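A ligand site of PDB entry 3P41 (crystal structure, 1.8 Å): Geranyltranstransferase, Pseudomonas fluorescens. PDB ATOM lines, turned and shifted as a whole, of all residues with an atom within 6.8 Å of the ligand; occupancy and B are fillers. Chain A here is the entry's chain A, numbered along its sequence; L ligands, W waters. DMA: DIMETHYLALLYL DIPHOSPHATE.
NH1 of Arg 55 sits close to NE2 of His 84 (3.4 Å).
The guanidinium group (NH1) of Arg 53 is in salt-bridge range of the side-chain carboxylate (OE2) of Glu 81, at 2.9 Å.
OD1 of Asn 49 is in hydrogen-bond range of N of Gly 51 (3.0 Å).
Gly 51 touches the ligand.
CD1 of Ile 193 touches C4 of the ligand, at 3.6 Å.
Phe 226 touches the ligand (CZ to O1, 3.5 Å).
Ile 298 touches the ligand (CD1 to C5, 3.5 Å).
Hydrophobic or aromatic side chains within 4 Å of the ligand: Val 54, His 84, Ile 193, Phe 226 and Ile 298.
Of the 22 residues printed, 10 come within 4 Å of the ligand.
NH2 of Arg 55 is in salt-bridge range of O2A of the ligand, 2.8 Å away.
N of Lys 52 sits at hydrogen-bond distance from O1B of the ligand (2.9 Å).
An oxygen (O2B) of the ligand sits at hydrogen-bond distance from a ring nitrogen (NE2) of His 84, at 2.9 Å.
The guanidinium group (NH1) of Arg 103 lies within salt-bridge range of an oxygen (O1A) of the ligand.
The backbone NH (N) of Val 54 sits at hydrogen-bond distance from an oxygen (O3B) of the ligand, 3.0 Å away.
N of Arg 53 is in hydrogen-bond range of O3B of the ligand (3.2 Å).
Water W4 lies within hydrogen-bond range of the side-chain carboxylate of Glu 81, an oxygen (O3B) of the ligand and the backbone NH of Arg 53.
Water W1 lies within hydrogen-bond range of O2A of the ligand (2.6 Å) and NH2 of Arg 55 (3.2 Å).
Water W2 lies within hydrogen-bond range of OE1 of Glu 81 (2.5 Å), O3B of the ligand (2.7 Å), N of Arg 55 (3.0 Å) and N of Val 54 (3.3 Å).
Water W5 lies within hydrogen-bond range of O2B of the ligand (2.9 Å), ND2 of Asn 49 (3.0 Å) and NE2 of His 84 (3.1 Å).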
ATOM      1  N   ASN A  49     -30.804  20.054  24.086  1.00  0.00           N
ATOM      2  CA  ASN A  49     -30.634  18.660  24.474  1.00  0.00           C
ATOM      3  C   ASN A  49     -29.533  18.461  25.517  1.00  0.00           C
ATOM      4  O   ASN A  49     -29.323  17.354  25.999  1.00  0.00           O
ATOM      5  CB  ASN A  49     -30.328  17.786  23.242  1.00  0.00           C
ATOM      6  CG  ASN A  49     -29.181  18.341  22.397  1.00  0.00           C
ATOM      7  OD1 ASN A  49     -28.338  19.118  22.883  1.00  0.00           O
ATOM      8  ND2 ASN A  49     -29.122  17.936  21.125  1.00  0.00           N
ATOM      9  N   GLY A  50     -28.828  19.546  25.847  1.00  0.00           N
ATOM     10  CA  GLY A  50     -27.781  19.521  26.856  1.00  0.00           C
ATOM     11  C   GLY A  50     -26.378  19.298  26.300  1.00  0.00           C
ATOM     12  O   GLY A  50     -25.430  19.162  27.078  1.00  0.00           O
ATOM     13  N   GLY A  51     -26.242  19.268  24.976  1.00  0.00           N
ATOM     14  CA  GLY A  51     -24.937  19.021  24.347  1.00  0.00           C
ATOM     15  C   GLY A  51     -23.937  20.162  24.455  1.00  0.00           C
ATOM     16  O   GLY A  51     -24.286  21.306  24.749  1.00  0.00           O
ATOM     17  N   LYS A  52     -22.670  19.883  24.178  1.00  0.00           N
ATOM     18  CA  LYS A  52     -21.632  20.902  24.296  1.00  0.00           C
ATOM     19  C   LYS A  52     -21.374  21.665  22.987  1.00  0.00           C
ATOM     20  O   LYS A  52     -20.422  22.433  22.904  1.00  0.00           O
ATOM     21  CB  LYS A  52     -20.337  20.241  24.801  1.00  0.00           C
ATOM     22  CG  LYS A  52     -20.514  19.505  26.117  1.00  0.00           C
ATOM     23  CD  LYS A  52     -20.783  20.475  27.263  1.00  0.00           C
ATOM     24  CE  LYS A  52     -19.649  21.498  27.375  1.00  0.00           C
ATOM     25  NZ  LYS A  52     -19.606  22.218  28.694  1.00  0.00           N
ATOM     26  N   ARG A  53     -22.221  21.468  21.972  1.00  0.00           N
ATOM     27  CA  ARG A  53     -22.057  22.085  20.647  1.00  0.00           C
ATOM     28  C   ARG A  53     -20.664  21.900  20.071  1.00  0.00           C
ATOM     29  O   ARG A  53     -20.062  22.869  19.603  1.00  0.00           O
ATOM     30  CB  ARG A  53     -22.320  23.589  20.696  1.00  0.00           C
ATOM     31  CG  ARG A  53     -23.568  24.006  21.476  1.00  0.00           C
ATOM     32  CD  ARG A  53     -24.801  23.403  20.882  1.00  0.00           C
ATOM     33  NE  ARG A  53     -25.967  23.990  21.548  1.00  0.00           N
ATOM     34  CZ  ARG A  53     -27.153  23.406  21.650  1.00  0.00           C
ATOM     35  NH1 ARG A  53     -27.361  22.203  21.124  1.00  0.00           N
ATOM     36  NH2 ARG A  53     -28.151  24.036  22.282  1.00  0.00           N
ATOM     37  N   VAL A  54     -20.137  20.691  20.160  1.00  0.00           N
ATOM     38  CA  VAL A  54     -18.767  20.465  19.723  1.00  0.00           C
ATOM     39  C   VAL A  54     -18.647  20.606  18.217  1.00  0.00           C
ATOM     40  O   VAL A  54     -17.603  20.969  17.703  1.00  0.00           O
ATOM     41  CB  VAL A  54     -18.287  19.079  20.128  1.00  0.00           C
ATOM     42  CG1 VAL A  54     -16.847  18.916  19.680  1.00  0.00           C
ATOM     43  CG2 VAL A  54     -18.408  18.892  21.633  1.00  0.00           C
ATOM     44  N   ARG A  55     -19.745  20.384  17.497  1.00  0.00           N
ATOM     45  CA  ARG A  55     -19.633  20.443  16.037  1.00  0.00           C
ATOM     46  C   ARG A  55     -19.521  21.892  15.559  1.00  0.00           C
ATOM     47  O   ARG A  55     -18.660  22.216  14.745  1.00  0.00           O
ATOM     48  CB  ARG A  55     -20.755  19.644  15.345  1.00  0.00           C
ATOM     49  CG  ARG A  55     -20.514  18.114  15.462  1.00  0.00           C
ATOM     50  CD  ARG A  55     -21.742  17.269  15.176  1.00  0.00           C
ATOM     51  NE  ARG A  55     -21.513  15.864  15.534  1.00  0.00           N
ATOM     52  CZ  ARG A  55     -21.506  15.385  16.777  1.00  0.00           C
ATOM     53  NH1 ARG A  55     -21.695  16.187  17.825  1.00  0.00           N
ATOM     54  NH2 ARG A  55     -21.266  14.083  16.993  1.00  0.00           N
ATOM     55  N   PRO A  56     -20.361  22.771  16.116  1.00  0.00           N
ATOM     56  CA  PRO A  56     -20.187  24.224  15.978  1.00  0.00           C
ATOM     57  C   PRO A  56     -18.799  24.670  16.421  1.00  0.00           C
ATOM     58  O   PRO A  56     -18.131  25.419  15.719  1.00  0.00           O
ATOM     59  CB  PRO A  56     -21.291  24.806  16.882  1.00  0.00           C
ATOM     60  CG  PRO A  56     -22.386  23.757  16.833  1.00  0.00           C
ATOM     61  CD  PRO A  56     -21.574  22.400  16.862  1.00  0.00           C
ATOM     62  N   LEU A  58     -16.100  23.025  16.296  1.00  0.00           N
ATOM     63  CA  LEU A  58     -15.262  22.640  15.165  1.00  0.00           C
ATOM     64  C   LEU A  58     -15.358  23.568  13.942  1.00  0.00           C
ATOM     65  O   LEU A  58     -14.335  23.953  13.421  1.00  0.00           O
ATOM     66  CB  LEU A  58     -15.532  21.178  14.773  1.00  0.00           C
ATOM     67  CG  LEU A  58     -14.929  20.142  15.738  1.00  0.00           C
ATOM     68  CD1 LEU A  58     -15.665  18.870  15.512  1.00  0.00           C
ATOM     69  CD2 LEU A  58     -13.367  19.982  15.577  1.00  0.00           C
ATOM     70  N   GLU A  81     -25.060  21.469  13.774  1.00  0.00           N
ATOM     71  CA  GLU A  81     -25.773  21.192  14.994  1.00  0.00           C
ATOM     72  C   GLU A  81     -27.226  20.748  14.757  1.00  0.00           C
ATOM     73  O   GLU A  81     -27.784  19.946  15.509  1.00  0.00           O
ATOM     74  CB  GLU A  81     -25.662  22.373  15.974  1.00  0.00           C
ATOM     75  CG  GLU A  81     -26.174  22.089  17.383  1.00  0.00           C
ATOM     76  CD  GLU A  81     -25.313  21.090  18.185  1.00  0.00           C
ATOM     77  OE1 GLU A  81     -24.181  20.797  17.734  1.00  0.00           O
ATOM     78  OE2 GLU A  81     -25.756  20.665  19.273  1.00  0.00           O
ATOM     79  N   HIS A  84     -27.004  17.205  13.642  1.00  0.00           N
ATOM     80  CA  HIS A  84     -26.755  16.409  14.842  1.00  0.00           C
ATOM     81  C   HIS A  84     -28.014  16.238  15.716  1.00  0.00           C
ATOM     82  O   HIS A  84     -28.393  15.129  16.114  1.00  0.00           O
ATOM     83  CB  HIS A  84     -25.552  17.013  15.596  1.00  0.00           C
ATOM     84  CG  HIS A  84     -25.252  16.349  16.902  1.00  0.00           C
ATOM     85  ND1 HIS A  84     -24.861  15.032  16.990  1.00  0.00           N
ATOM     86  CD2 HIS A  84     -25.275  16.825  18.176  1.00  0.00           C
ATOM     87  CE1 HIS A  84     -24.685  14.716  18.258  1.00  0.00           C
ATOM     88  NE2 HIS A  84     -24.911  15.788  18.999  1.00  0.00           N
ATOM     89  N   LEU A  88     -30.289  12.559  16.663  1.00  0.00           N
ATOM     90  CA  LEU A  88     -30.506  12.075  18.005  1.00  0.00           C
ATOM     91  C   LEU A  88     -31.995  11.852  18.244  1.00  0.00           C
ATOM     92  O   LEU A  88     -32.410  10.865  18.839  1.00  0.00           O
ATOM     93  CB  LEU A  88     -29.945  13.076  19.031  1.00  0.00           C
ATOM     94  CG  LEU A  88     -28.446  13.380  18.953  1.00  0.00           C
ATOM     95  CD1 LEU A  88     -28.106  14.435  20.005  1.00  0.00           C
ATOM     96  CD2 LEU A  88     -27.627  12.118  19.140  1.00  0.00           C
ATOM     97  N   ARG A 103     -29.143  12.394  28.277  1.00  0.00           N
ATOM     98  CA  ARG A 103     -28.431  13.337  29.101  1.00  0.00           C
ATOM     99  C   ARG A 103     -29.284  13.779  30.270  1.00  0.00           C
ATOM    100  O   ARG A 103     -29.296  14.908  30.610  1.00  0.00           O
ATOM    101  CB  ARG A 103     -27.922  14.511  28.288  1.00  0.00           C
ATOM    102  CG  ARG A 103     -26.670  14.159  27.486  1.00  0.00           C
ATOM    103  CD  ARG A 103     -25.998  15.377  26.927  1.00  0.00           C
ATOM    104  NE  ARG A 103     -24.643  15.088  26.470  1.00  0.00           N
ATOM    105  CZ  ARG A 103     -24.284  15.117  25.200  1.00  0.00           C
ATOM    106  NH1 ARG A 103     -23.040  14.879  24.869  1.00  0.00           N
ATOM    107  NH2 ARG A 103     -25.198  15.034  24.265  1.00  0.00           N
ATOM    108  N   THR A 189     -20.502   8.762  12.913  1.00  0.00           N
ATOM    109  CA  THR A 189     -20.069  10.033  13.503  1.00  0.00           C
ATOM    110  C   THR A 189     -18.917  10.732  12.743  1.00  0.00           C
ATOM    111  O   THR A 189     -18.828  11.941  12.764  1.00  0.00           O
ATOM    112  CB  THR A 189     -19.668   9.859  14.975  1.00  0.00           C
ATOM    113  OG1 THR A 189     -18.650   8.857  15.081  1.00  0.00           O
ATOM    114  CG2 THR A 189     -20.864   9.494  15.847  1.00  0.00           C
ATOM    115  N   ILE A 193     -18.456  15.002  11.645  1.00  0.00           N
ATOM    116  CA  ILE A 193     -17.316  15.688  12.228  1.00  0.00           C
ATOM    117  C   ILE A 193     -16.417  16.315  11.153  1.00  0.00           C
ATOM    118  O   ILE A 193     -16.071  17.497  11.241  1.00  0.00           O
ATOM    119  CB  ILE A 193     -16.551  14.748  13.199  1.00  0.00           C
ATOM    120  CG1 ILE A 193     -17.422  14.514  14.448  1.00  0.00           C
ATOM    121  CG2 ILE A 193     -15.163  15.319  13.535  1.00  0.00           C
ATOM    122  CD1 ILE A 193     -16.905  13.392  15.354  1.00  0.00           C
ATOM    123  N   SER A 196     -18.087  19.249   9.710  1.00  0.00           N
ATOM    124  CA  SER A 196     -17.969  20.393  10.595  1.00  0.00           C
ATOM    125  C   SER A 196     -16.721  21.240  10.286  1.00  0.00           C
ATOM    126  O   SER A 196     -16.805  22.442  10.033  1.00  0.00           O
ATOM    127  CB  SER A 196     -18.025  19.974  12.064  1.00  0.00           C
ATOM    128  OG  SER A 196     -19.255  19.347  12.383  1.00  0.00           O
ATOM    129  N   ILE A 222      -9.669  12.747  15.055  1.00  0.00           N
ATOM    130  CA  ILE A 222     -10.406  12.998  16.290  1.00  0.00           C
ATOM    131  C   ILE A 222     -11.733  12.258  16.359  1.00  0.00           C
ATOM    132  O   ILE A 222     -12.182  11.917  17.460  1.00  0.00           O
ATOM    133  CB  ILE A 222     -10.619  14.517  16.613  1.00  0.00           C
ATOM    134  CG1 ILE A 222     -11.557  15.179  15.587  1.00  0.00           C
ATOM    135  CG2 ILE A 222      -9.271  15.239  16.779  1.00  0.00           C
ATOM    136  CD1 ILE A 222     -12.168  16.542  16.074  1.00  0.00           C
ATOM    137  N   GLY A 223     -12.353  12.026  15.201  1.00  0.00           N
ATOM    138  CA  GLY A 223     -13.653  11.328  15.163  1.00  0.00           C
ATOM    139  C   GLY A 223     -13.512   9.911  15.706  1.00  0.00           C
ATOM    140  O   GLY A 223     -14.343   9.440  16.471  1.00  0.00           O
ATOM    141  N   PHE A 226     -12.412   9.918  19.566  1.00  0.00           N
ATOM    142  CA  PHE A 226     -13.565  10.018  20.424  1.00  0.00           C
ATOM    143  C   PHE A 226     -14.257   8.667  20.717  1.00  0.00           C
ATOM    144  O   PHE A 226     -14.698   8.403  21.845  1.00  0.00           O
ATOM    145  CB  PHE A 226     -14.583  10.971  19.782  1.00  0.00           C
ATOM    146  CG  PHE A 226     -15.854  11.054  20.531  1.00  0.00           C
ATOM    147  CD1 PHE A 226     -17.002  10.461  20.032  1.00  0.00           C
ATOM    148  CD2 PHE A 226     -15.883  11.677  21.765  1.00  0.00           C
ATOM    149  CE1 PHE A 226     -18.190  10.530  20.746  1.00  0.00           C
ATOM    150  CE2 PHE A 226     -17.073  11.748  22.489  1.00  0.00           C
ATOM    151  CZ  PHE A 226     -18.224  11.167  21.976  1.00  0.00           C
ATOM    152  N   ASP A 230     -14.458   6.758  24.163  1.00  0.00           N
ATOM    153  CA  ASP A 230     -15.781   6.460  24.722  1.00  0.00           C
ATOM    154  C   ASP A 230     -15.803   5.031  25.293  1.00  0.00           C
ATOM    155  O   ASP A 230     -16.223   4.815  26.435  1.00  0.00           O
ATOM    156  CB  ASP A 230     -16.873   6.586  23.685  1.00  0.00           C
ATOM    157  CG  ASP A 230     -17.713   7.824  23.882  1.00  0.00           C
ATOM    158  OD1 ASP A 230     -17.309   8.720  24.645  1.00  0.00           O
ATOM    159  OD2 ASP A 230     -18.798   7.879  23.252  1.00  0.00           O
ATOM    160  N   LEU A 294      -8.724  20.586  21.662  1.00  0.00           N
ATOM    161  CA  LEU A 294      -9.820  19.607  21.620  1.00  0.00           C
ATOM    162  C   LEU A 294      -9.260  18.177  21.417  1.00  0.00           C
ATOM    163  O   LEU A 294      -9.696  17.217  22.055  1.00  0.00           O
ATOM    164  CB  LEU A 294     -10.763  19.903  20.470  1.00  0.00           C
ATOM    165  CG  LEU A 294     -12.016  19.029  20.309  1.00  0.00           C
ATOM    166  CD1 LEU A 294     -13.006  19.197  21.428  1.00  0.00           C
ATOM    167  CD2 LEU A 294     -12.653  19.365  18.953  1.00  0.00           C
ATOM    168  N   ILE A 298     -10.104  15.152  24.146  1.00  0.00           N
ATOM    169  CA  ILE A 298     -10.902  13.990  23.796  1.00  0.00           C
ATOM    170  C   ILE A 298     -10.294  12.713  24.365  1.00  0.00           C
ATOM    171  O   ILE A 298     -11.019  11.843  24.835  1.00  0.00           O
ATOM    172  CB  ILE A 298     -11.063  13.925  22.266  1.00  0.00           C
ATOM    173  CG1 ILE A 298     -12.153  14.942  21.846  1.00  0.00           C
ATOM    174  CG2 ILE A 298     -11.417  12.511  21.799  1.00  0.00           C
ATOM    175  CD1 ILE A 298     -12.305  15.070  20.341  1.00  0.00           C
HETATM  176  C1  DMA L   1     -18.783  14.996  20.007  1.00  0.00           C
HETATM  177  O1  DMA L   1     -19.409  14.374  21.104  1.00  0.00           O
HETATM  178  C2  DMA L   1     -17.357  14.580  19.865  1.00  0.00           C
HETATM  179  C3  DMA L   1     -16.743  15.051  18.785  1.00  0.00           C
HETATM  180  C4  DMA L   1     -17.520  15.908  17.829  1.00  0.00           C
HETATM  181  C5  DMA L   1     -15.309  14.719  18.514  1.00  0.00           C
HETATM  182  PA  DMA L   1     -21.012  14.564  21.129  1.00  0.00           P
HETATM  183  O1A DMA L   1     -21.586  13.956  22.407  1.00  0.00           O
HETATM  184  O2A DMA L   1     -21.512  14.033  19.812  1.00  0.00           O
HETATM  185  O3A DMA L   1     -21.082  16.184  21.104  1.00  0.00           O
HETATM  186  PB  DMA L   1     -22.228  17.142  21.709  1.00  0.00           P
HETATM  187  O1B DMA L   1     -21.887  17.286  23.191  1.00  0.00           O
HETATM  188  O2B DMA L   1     -23.525  16.352  21.483  1.00  0.00           O
HETATM  189  O3B DMA L   1     -22.049  18.450  20.919  1.00  0.00           O
HETATM  190  O   HOH W   1     -21.703  11.604  18.914  1.00  0.00           O
HETATM  191  O   HOH W   2     -22.390  19.183  18.323  1.00  0.00           O
HETATM  192  O   HOH W   3     -24.210  12.851  21.360  1.00  0.00           O
HETATM  193  O   HOH W   4     -24.284  19.694  21.004  1.00  0.00           O
HETATM  194  O   HOH W   5     -26.279  17.164  21.436  1.00  0.00           O
